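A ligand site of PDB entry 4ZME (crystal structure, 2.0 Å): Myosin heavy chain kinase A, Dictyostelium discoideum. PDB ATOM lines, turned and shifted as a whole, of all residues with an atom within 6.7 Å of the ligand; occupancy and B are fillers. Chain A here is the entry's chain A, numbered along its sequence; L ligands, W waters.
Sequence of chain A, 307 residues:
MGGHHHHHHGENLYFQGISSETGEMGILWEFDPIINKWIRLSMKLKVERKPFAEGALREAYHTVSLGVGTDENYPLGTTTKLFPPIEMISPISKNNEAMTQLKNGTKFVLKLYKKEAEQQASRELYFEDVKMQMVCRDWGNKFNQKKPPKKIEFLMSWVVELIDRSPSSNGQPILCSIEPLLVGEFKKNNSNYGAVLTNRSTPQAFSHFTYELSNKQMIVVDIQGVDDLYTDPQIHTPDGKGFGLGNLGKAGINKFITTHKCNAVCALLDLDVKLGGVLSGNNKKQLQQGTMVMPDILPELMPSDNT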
ATOM      1  N   PHE A  52     -30.261  26.832  24.768  1.00  0.00           N
ATOM      2  CA  PHE A  52     -31.138  27.795  24.099  1.00  0.00           C
ATOM      3  C   PHE A  52     -32.047  27.158  23.043  1.00  0.00           C
ATOM      4  O   PHE A  52     -32.890  27.836  22.459  1.00  0.00           O
ATOM      5  CB  PHE A  52     -30.341  28.928  23.434  1.00  0.00           C
ATOM      6  CG  PHE A  52     -29.565  28.518  22.188  1.00  0.00           C
ATOM      7  CD1 PHE A  52     -28.275  27.996  22.289  1.00  0.00           C
ATOM      8  CD2 PHE A  52     -30.113  28.695  20.929  1.00  0.00           C
ATOM      9  CE1 PHE A  52     -27.560  27.626  21.166  1.00  0.00           C
ATOM     10  CE2 PHE A  52     -29.401  28.321  19.792  1.00  0.00           C
ATOM     11  CZ  PHE A  52     -28.122  27.802  19.909  1.00  0.00           C
ATOM     12  N   ALA A  53     -31.872  25.876  22.796  1.00  0.00           N
ATOM     13  CA  ALA A  53     -32.690  25.169  21.810  1.00  0.00           C
ATOM     14  C   ALA A  53     -32.521  23.694  21.991  1.00  0.00           C
ATOM     15  O   ALA A  53     -31.587  23.237  22.660  1.00  0.00           O
ATOM     16  CB  ALA A  53     -32.275  25.577  20.401  1.00  0.00           C
ATOM     17  N   GLU A  54     -33.421  22.917  21.389  1.00  0.00           N
ATOM     18  CA  GLU A  54     -33.272  21.469  21.397  1.00  0.00           C
ATOM     19  C   GLU A  54     -33.857  20.815  20.170  1.00  0.00           C
ATOM     20  O   GLU A  54     -34.752  21.369  19.522  1.00  0.00           O
ATOM     21  CB  GLU A  54     -33.863  20.861  22.652  1.00  0.00           C
ATOM     22  CG  GLU A  54     -35.360  20.988  22.770  1.00  0.00           C
ATOM     23  CD  GLU A  54     -35.960  19.996  23.757  1.00  0.00           C
ATOM     24  OE1 GLU A  54     -35.199  19.216  24.388  1.00  0.00           O
ATOM     25  OE2 GLU A  54     -37.196  19.988  23.895  1.00  0.00           O
ATOM     26  N   GLY A  55     -33.330  19.644  19.845  1.00  0.00           N
ATOM     27  CA  GLY A  55     -33.833  18.822  18.753  1.00  0.00           C
ATOM     28  C   GLY A  55     -34.340  17.530  19.352  1.00  0.00           C
ATOM     29  O   GLY A  55     -34.603  17.439  20.555  1.00  0.00           O
ATOM     30  N   ALA A  56     -34.484  16.510  18.506  1.00  0.00           N
ATOM     31  CA  ALA A  56     -34.977  15.223  18.950  1.00  0.00           C
ATOM     32  C   ALA A  56     -34.086  14.600  20.014  1.00  0.00           C
ATOM     33  O   ALA A  56     -34.580  14.070  21.009  1.00  0.00           O
ATOM     34  CB  ALA A  56     -35.099  14.284  17.748  1.00  0.00           C
ATOM     35  N   ARG A  58     -30.619  16.014  20.951  1.00  0.00           N
ATOM     36  CA  ARG A  58     -29.565  16.855  21.516  1.00  0.00           C
ATOM     37  C   ARG A  58     -30.103  18.214  21.906  1.00  0.00           C
ATOM     38  O   ARG A  58     -31.112  18.675  21.383  1.00  0.00           O
ATOM     39  CB  ARG A  58     -28.422  17.030  20.512  1.00  0.00           C
ATOM     40  CG  ARG A  58     -27.671  15.765  20.186  1.00  0.00           C
ATOM     41  CD  ARG A  58     -26.573  16.001  19.161  1.00  0.00           C
ATOM     42  NE  ARG A  58     -27.111  16.438  17.880  1.00  0.00           N
ATOM     43  CZ  ARG A  58     -26.397  16.825  16.840  1.00  0.00           C
ATOM     44  NH1 ARG A  58     -25.068  16.845  16.894  1.00  0.00           N
ATOM     45  NH2 ARG A  58     -27.001  17.237  15.743  1.00  0.00           N
ATOM     46  N   ALA A  60     -28.757  22.387  22.426  1.00  0.00           N
ATOM     47  CA  ALA A  60     -27.716  23.333  22.059  1.00  0.00           C
ATOM     48  C   ALA A  60     -27.493  24.364  23.139  1.00  0.00           C
ATOM     49  O   ALA A  60     -28.444  24.921  23.691  1.00  0.00           O
ATOM     50  CB  ALA A  60     -28.086  24.018  20.751  1.00  0.00           C
ATOM     51  N   HIS A  62     -25.175  27.926  24.224  1.00  0.00           N
ATOM     52  CA  HIS A  62     -24.228  28.992  23.913  1.00  0.00           C
ATOM     53  C   HIS A  62     -22.943  28.841  24.719  1.00  0.00           C
ATOM     54  O   HIS A  62     -22.965  28.541  25.918  1.00  0.00           O
ATOM     55  CB  HIS A  62     -24.824  30.371  24.192  1.00  0.00           C
ATOM     56  CG  HIS A  62     -25.892  30.769  23.232  1.00  0.00           C
ATOM     57  ND1 HIS A  62     -25.667  30.902  21.877  1.00  0.00           N
ATOM     58  CD2 HIS A  62     -27.197  31.087  23.429  1.00  0.00           C
ATOM     59  CE1 HIS A  62     -26.782  31.271  21.281  1.00  0.00           C
ATOM     60  NE2 HIS A  62     -27.722  31.394  22.197  1.00  0.00           N
ATOM     61  N   VAL A 109     -21.484  27.326  19.412  1.00  0.00           N
ATOM     62  CA  VAL A 109     -22.554  26.463  19.854  1.00  0.00           C
ATOM     63  C   VAL A 109     -22.004  25.087  20.237  1.00  0.00           C
ATOM     64  O   VAL A 109     -21.222  24.487  19.491  1.00  0.00           O
ATOM     65  CB  VAL A 109     -23.620  26.300  18.759  1.00  0.00           C
ATOM     66  CG1 VAL A 109     -24.688  25.270  19.136  1.00  0.00           C
ATOM     67  CG2 VAL A 109     -24.290  27.645  18.495  1.00  0.00           C
ATOM     68  N   LYS A 111     -23.324  21.131  21.390  1.00  0.00           N
ATOM     69  CA  LYS A 111     -24.466  20.221  21.382  1.00  0.00           C
ATOM     70  C   LYS A 111     -24.180  18.962  22.189  1.00  0.00           C
ATOM     71  O   LYS A 111     -23.141  18.335  22.009  1.00  0.00           O
ATOM     72  CB  LYS A 111     -24.837  19.841  19.954  1.00  0.00           C
ATOM     73  CG  LYS A 111     -25.223  21.059  19.131  1.00  0.00           C
ATOM     74  CD  LYS A 111     -25.764  20.699  17.774  1.00  0.00           C
ATOM     75  CE  LYS A 111     -25.950  21.971  16.963  1.00  0.00           C
ATOM     76  NZ  LYS A 111     -26.380  21.715  15.553  1.00  0.00           N
ATOM     77  N   LEU A 155     -20.898  24.711   7.837  1.00  0.00           N
ATOM     78  CA  LEU A 155     -20.017  25.079   8.928  1.00  0.00           C
ATOM     79  C   LEU A 155     -19.039  23.943   9.240  1.00  0.00           C
ATOM     80  O   LEU A 155     -19.368  22.788   9.056  1.00  0.00           O
ATOM     81  CB  LEU A 155     -20.836  25.348  10.184  1.00  0.00           C
ATOM     82  CG  LEU A 155     -21.845  26.497  10.227  1.00  0.00           C
ATOM     83  CD1 LEU A 155     -22.539  26.468  11.588  1.00  0.00           C
ATOM     84  CD2 LEU A 155     -21.161  27.845   9.989  1.00  0.00           C
ATOM     85  N   GLU A 179     -19.711  23.816  17.089  1.00  0.00           N
ATOM     86  CA  GLU A 179     -19.732  24.418  15.756  1.00  0.00           C
ATOM     87  C   GLU A 179     -19.954  25.910  15.887  1.00  0.00           C
ATOM     88  O   GLU A 179     -20.340  26.350  16.951  1.00  0.00           O
ATOM     89  CB  GLU A 179     -20.815  23.787  14.898  1.00  0.00           C
ATOM     90  CG  GLU A 179     -22.215  24.010  15.474  1.00  0.00           C
ATOM     91  CD  GLU A 179     -23.257  23.106  14.869  1.00  0.00           C
ATOM     92  OE1 GLU A 179     -24.204  23.613  14.230  1.00  0.00           O
ATOM     93  OE2 GLU A 179     -23.160  21.887  15.056  1.00  0.00           O
ATOM     94  N   PRO A 180     -19.702  26.679  14.825  1.00  0.00           N
ATOM     95  CA  PRO A 180     -19.900  28.127  14.907  1.00  0.00           C
ATOM     96  C   PRO A 180     -21.337  28.505  15.119  1.00  0.00           C
ATOM     97  O   PRO A 180     -22.239  27.696  14.852  1.00  0.00           O
ATOM     98  CB  PRO A 180     -19.420  28.621  13.542  1.00  0.00           C
ATOM     99  CG  PRO A 180     -18.441  27.601  13.082  1.00  0.00           C
ATOM    100  CD  PRO A 180     -19.058  26.304  13.549  1.00  0.00           C
ATOM    101  N   LEU A 181     -21.529  29.711  15.636  1.00  0.00           N
ATOM    102  CA  LEU A 181     -22.862  30.237  15.933  1.00  0.00           C
ATOM    103  C   LEU A 181     -23.482  30.804  14.665  1.00  0.00           C
ATOM    104  O   LEU A 181     -22.879  31.639  14.018  1.00  0.00           O
ATOM    105  CB  LEU A 181     -22.770  31.354  16.973  1.00  0.00           C
ATOM    106  CG  LEU A 181     -24.079  32.117  17.238  1.00  0.00           C
ATOM    107  CD1 LEU A 181     -25.136  31.204  17.815  1.00  0.00           C
ATOM    108  CD2 LEU A 181     -23.843  33.310  18.155  1.00  0.00           C
ATOM    109  N   LEU A 182     -24.654  30.315  14.294  1.00  0.00           N
ATOM    110  CA  LEU A 182     -25.394  30.911  13.208  1.00  0.00           C
ATOM    111  C   LEU A 182     -26.254  32.048  13.746  1.00  0.00           C
ATOM    112  O   LEU A 182     -27.026  31.850  14.678  1.00  0.00           O
ATOM    113  CB  LEU A 182     -26.308  29.887  12.534  1.00  0.00           C
ATOM    114  CG  LEU A 182     -25.592  28.786  11.742  1.00  0.00           C
ATOM    115  CD1 LEU A 182     -26.611  27.740  11.347  1.00  0.00           C
ATOM    116  CD2 LEU A 182     -24.904  29.331  10.509  1.00  0.00           C
ATOM    117  N   VAL A 183     -26.117  33.227  13.158  1.00  0.00           N
ATOM    118  CA  VAL A 183     -27.012  34.348  13.495  1.00  0.00           C
ATOM    119  C   VAL A 183     -28.082  34.554  12.434  1.00  0.00           C
ATOM    120  O   VAL A 183     -27.770  34.823  11.269  1.00  0.00           O
ATOM    121  CB  VAL A 183     -26.222  35.650  13.702  1.00  0.00           C
ATOM    122  CG1 VAL A 183     -27.129  36.683  14.365  1.00  0.00           C
ATOM    123  CG2 VAL A 183     -25.009  35.395  14.577  1.00  0.00           C
ATOM    124  N   GLY A 184     -29.339  34.425  12.836  1.00  0.00           N
ATOM    125  CA  GLY A 184     -30.475  34.629  11.929  1.00  0.00           C
ATOM    126  C   GLY A 184     -31.546  33.594  12.127  1.00  0.00           C
ATOM    127  O   GLY A 184     -31.521  32.820  13.080  1.00  0.00           O
ATOM    128  N   PHE A 186     -33.158  30.245  11.654  1.00  0.00           N
ATOM    129  CA  PHE A 186     -32.743  28.894  11.348  1.00  0.00           C
ATOM    130  C   PHE A 186     -33.923  28.134  10.760  1.00  0.00           C
ATOM    131  O   PHE A 186     -34.995  28.104  11.356  1.00  0.00           O
ATOM    132  CB  PHE A 186     -32.276  28.203  12.628  1.00  0.00           C
ATOM    133  CG  PHE A 186     -31.506  26.918  12.396  1.00  0.00           C
ATOM    134  CD1 PHE A 186     -32.174  25.747  12.051  1.00  0.00           C
ATOM    135  CD2 PHE A 186     -30.123  26.864  12.596  1.00  0.00           C
ATOM    136  CE1 PHE A 186     -31.482  24.564  11.879  1.00  0.00           C
ATOM    137  CE2 PHE A 186     -29.433  25.677  12.411  1.00  0.00           C
ATOM    138  CZ  PHE A 186     -30.113  24.532  12.051  1.00  0.00           C
ATOM    139  N   LYS A 187     -33.745  27.569   9.566  1.00  0.00           N
ATOM    140  CA  LYS A 187     -34.808  26.816   8.913  1.00  0.00           C
ATOM    141  C   LYS A 187     -34.304  25.484   8.391  1.00  0.00           C
ATOM    142  O   LYS A 187     -33.214  25.405   7.844  1.00  0.00           O
ATOM    143  CB  LYS A 187     -35.366  27.586   7.726  1.00  0.00           C
ATOM    144  CG  LYS A 187     -36.084  28.877   8.083  1.00  0.00           C
ATOM    145  CD  LYS A 187     -36.942  29.399   6.950  1.00  0.00           C
ATOM    146  CE  LYS A 187     -36.275  29.159   5.587  1.00  0.00           C
ATOM    147  NZ  LYS A 187     -37.177  29.147   4.394  1.00  0.00           N
ATOM    148  N   LYS A 188     -35.108  24.444   8.587  1.00  0.00           N
ATOM    149  CA  LYS A 188     -34.853  23.134   8.013  1.00  0.00           C
ATOM    150  C   LYS A 188     -35.546  23.026   6.653  1.00  0.00           C
ATOM    151  O   LYS A 188     -36.714  23.384   6.514  1.00  0.00           O
ATOM    152  CB  LYS A 188     -35.343  22.064   8.971  1.00  0.00           C
ATOM    153  CG  LYS A 188     -34.807  20.680   8.635  1.00  0.00           C
ATOM    154  CD  LYS A 188     -35.343  19.635   9.592  1.00  0.00           C
ATOM    155  CE  LYS A 188     -34.582  18.349   9.430  1.00  0.00           C
ATOM    156  NZ  LYS A 188     -35.133  17.282  10.292  1.00  0.00           N
ATOM    157  N   GLN A 224     -30.244  22.168   6.400  1.00  0.00           N
ATOM    158  CA  GLN A 224     -30.795  23.109   7.349  1.00  0.00           C
ATOM    159  C   GLN A 224     -29.744  24.107   7.777  1.00  0.00           C
ATOM    160  O   GLN A 224     -28.528  23.786   7.844  1.00  0.00           O
ATOM    161  CB  GLN A 224     -31.325  22.356   8.553  1.00  0.00           C
ATOM    162  CG  GLN A 224     -30.302  21.482   9.237  1.00  0.00           C
ATOM    163  CD  GLN A 224     -30.888  20.618  10.321  1.00  0.00           C
ATOM    164  OE1 GLN A 224     -31.796  21.045  11.047  1.00  0.00           O
ATOM    165  NE2 GLN A 224     -30.386  19.380  10.462  1.00  0.00           N
ATOM    166  N   VAL A 226     -29.105  28.744   8.278  1.00  0.00           N
ATOM    167  CA  VAL A 226     -29.607  30.092   7.950  1.00  0.00           C
ATOM    168  C   VAL A 226     -29.142  30.535   6.596  1.00  0.00           C
ATOM    169  O   VAL A 226     -27.948  30.644   6.392  1.00  0.00           O
ATOM    170  CB  VAL A 226     -29.100  31.137   8.974  1.00  0.00           C
ATOM    171  CG1 VAL A 226     -29.614  32.533   8.601  1.00  0.00           C
ATOM    172  CG2 VAL A 226     -29.562  30.764  10.378  1.00  0.00           C
ATOM    173  N   THR A 231     -25.766  23.406   8.487  1.00  0.00           N
ATOM    174  CA  THR A 231     -25.154  22.618   9.529  1.00  0.00           C
ATOM    175  C   THR A 231     -25.981  21.369   9.778  1.00  0.00           C
ATOM    176  O   THR A 231     -27.122  21.247   9.314  1.00  0.00           O
ATOM    177  CB  THR A 231     -24.943  23.424  10.838  1.00  0.00           C
ATOM    178  OG1 THR A 231     -24.052  22.716  11.704  1.00  0.00           O
ATOM    179  CG2 THR A 231     -26.250  23.694  11.550  1.00  0.00           C
ATOM    180  N   PHD A 232     -25.369  20.415  10.461  1.00  0.00           N
ATOM    181  CA  PHD A 232     -25.995  19.129  10.767  1.00  0.00           C
ATOM    182  C   PHD A 232     -26.697  18.481   9.615  1.00  0.00           C
ATOM    183  O   PHD A 232     -27.882  18.152   9.719  1.00  0.00           O
ATOM    184  CB  PHD A 232     -27.014  19.360  11.893  1.00  0.00           C
ATOM    185  CG  PHD A 232     -27.587  18.078  12.453  1.00  0.00           C
ATOM    186  OD1 PHD A 232     -26.968  16.791  12.223  1.00  0.00           O
ATOM    187  OD2 PHD A 232     -28.599  18.174  13.119  1.00  0.00           O
ATOM    188  P   PHD A 232     -27.595  15.356  11.659  1.00  0.00           P
ATOM    189  OP1 PHD A 232     -26.383  14.501  11.213  1.00  0.00           O
ATOM    190  OP2 PHD A 232     -28.092  14.864  12.935  1.00  0.00           O
ATOM    191  OP3 PHD A 232     -28.646  15.646  10.582  1.00  0.00           O
HETATM  192  O1  LIG L   1     -32.938  21.781  17.121  1.00  0.00           O
HETATM  193  C1  LIG L   1     -31.940  22.416  16.330  1.00  0.00           C
HETATM  194  C2  LIG L   1     -32.042  23.884  16.632  1.00  0.00           C
HETATM  195  O2  LIG L   1     -30.889  24.383  17.343  1.00  0.00           O
HETATM  196  C3  LIG L   1     -32.179  24.676  15.350  1.00  0.00           C
HETATM  197  O3  LIG L   1     -33.544  24.812  14.969  1.00  0.00           O
HETATM  198  C4  LIG L   1     -31.564  25.993  15.715  1.00  0.00           C
HETATM  199  O4  LIG L   1     -32.568  26.852  16.278  1.00  0.00           O
HETATM  200  C5  LIG L   1     -30.504  25.630  16.725  1.00  0.00           C
HETATM  201  N1  LIG L   1     -29.156  25.479  16.133  1.00  0.00           N
HETATM  202  C6  LIG L   1     -28.538  24.340  15.731  1.00  0.00           C
HETATM  203  N2  LIG L   1     -27.264  24.606  15.288  1.00  0.00           N
HETATM  204  C7  LIG L   1     -27.074  25.926  15.422  1.00  0.00           C
HETATM  205  C8  LIG L   1     -25.978  26.894  15.167  1.00  0.00           C
HETATM  206  N3  LIG L   1     -24.797  26.500  14.653  1.00  0.00           N
HETATM  207  N4  LIG L   1     -26.204  28.194  15.462  1.00  0.00           N
HETATM  208  C9  LIG L   1     -27.384  28.638  15.966  1.00  0.00           C
HETATM  209  N5  LIG L   1     -28.400  27.817  16.212  1.00  0.00           N
HETATM  210  C10 LIG L   1     -28.315  26.492  15.970  1.00  0.00           C
HETATM  211  O   HOH W   1     -34.962  23.588  13.096  1.00  0.00           O
HETATM  212  O   HOH W   2     -30.496  29.599  16.410  1.00  0.00           O
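The backbone carbonyl oxygen (O) of Pro 180 lies within hydrogen-bond range of a nitrogen (N3) of the ligand (2.8 Å). A nitrogen (N4) of the ligand sits at hydrogen-bond distance from the backbone NH (N) of Leu 182, at 2.9 Å. The side-chain carboxylate of Glu 179 sits at hydrogen-bond distance from a nitrogen (N3) of the ligand. The side-chain amino group (NZ) of Lys 111 lies within hydrogen-bond range of a nitrogen (N2) of the ligand, 3.0 Å away. O of Glu 54 lies within hydrogen-bond range of O1 of the ligand, 3.0 Å away. The backbone NH (N) of Gly 55 is in hydrogen-bond range of an oxygen (O1) of the ligand (3.5 Å).
The side-chain carboxylate of Glu 179 is in salt-bridge range of the side-chain amino group of Lys 111 (3.2 Å). O of Glu 179 lies within hydrogen-bond range of N of Val 109 (2.9 Å). The side-chain hydroxyl (OG1) of Thr 231 sits at hydrogen-bond distance from the side-chain carboxylate (OE1) of Glu 179, at 2.7 Å. The backbone carbonyl oxygen (O) of Ala 53 lies within hydrogen-bond range of the backbone NH (N) of Ala 60 (3.0 Å). O of Ala 60 sits at hydrogen-bond distance from N of Phe 52. The backbone NH (N) of Thr 231 lies within hydrogen-bond range of the backbone carbonyl oxygen (O) of Gln 224, 2.9 Å away.
Phe 52 touches the ligand. Ala 53 touches the ligand (CB to O2, 3.6 Å). Val 109 touches the ligand. CD1 of Leu 155 touches N3 of the ligand (3.8 Å). Leu 181 touches the ligand. CD1 of Phe 186 touches O3 of the ligand, at 3.4 Å. Thr 231 touches the ligand (CG2 to N2, 3.98 Å). Hydrophobic or aromatic side chains within 4 Å of the ligand: Phe 52, Ala 53, Val 109, Leu 155, Leu 181, Leu 182 and Phe 186. Of the 24 residues printed, 13 come within 4 Å of the ligand.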
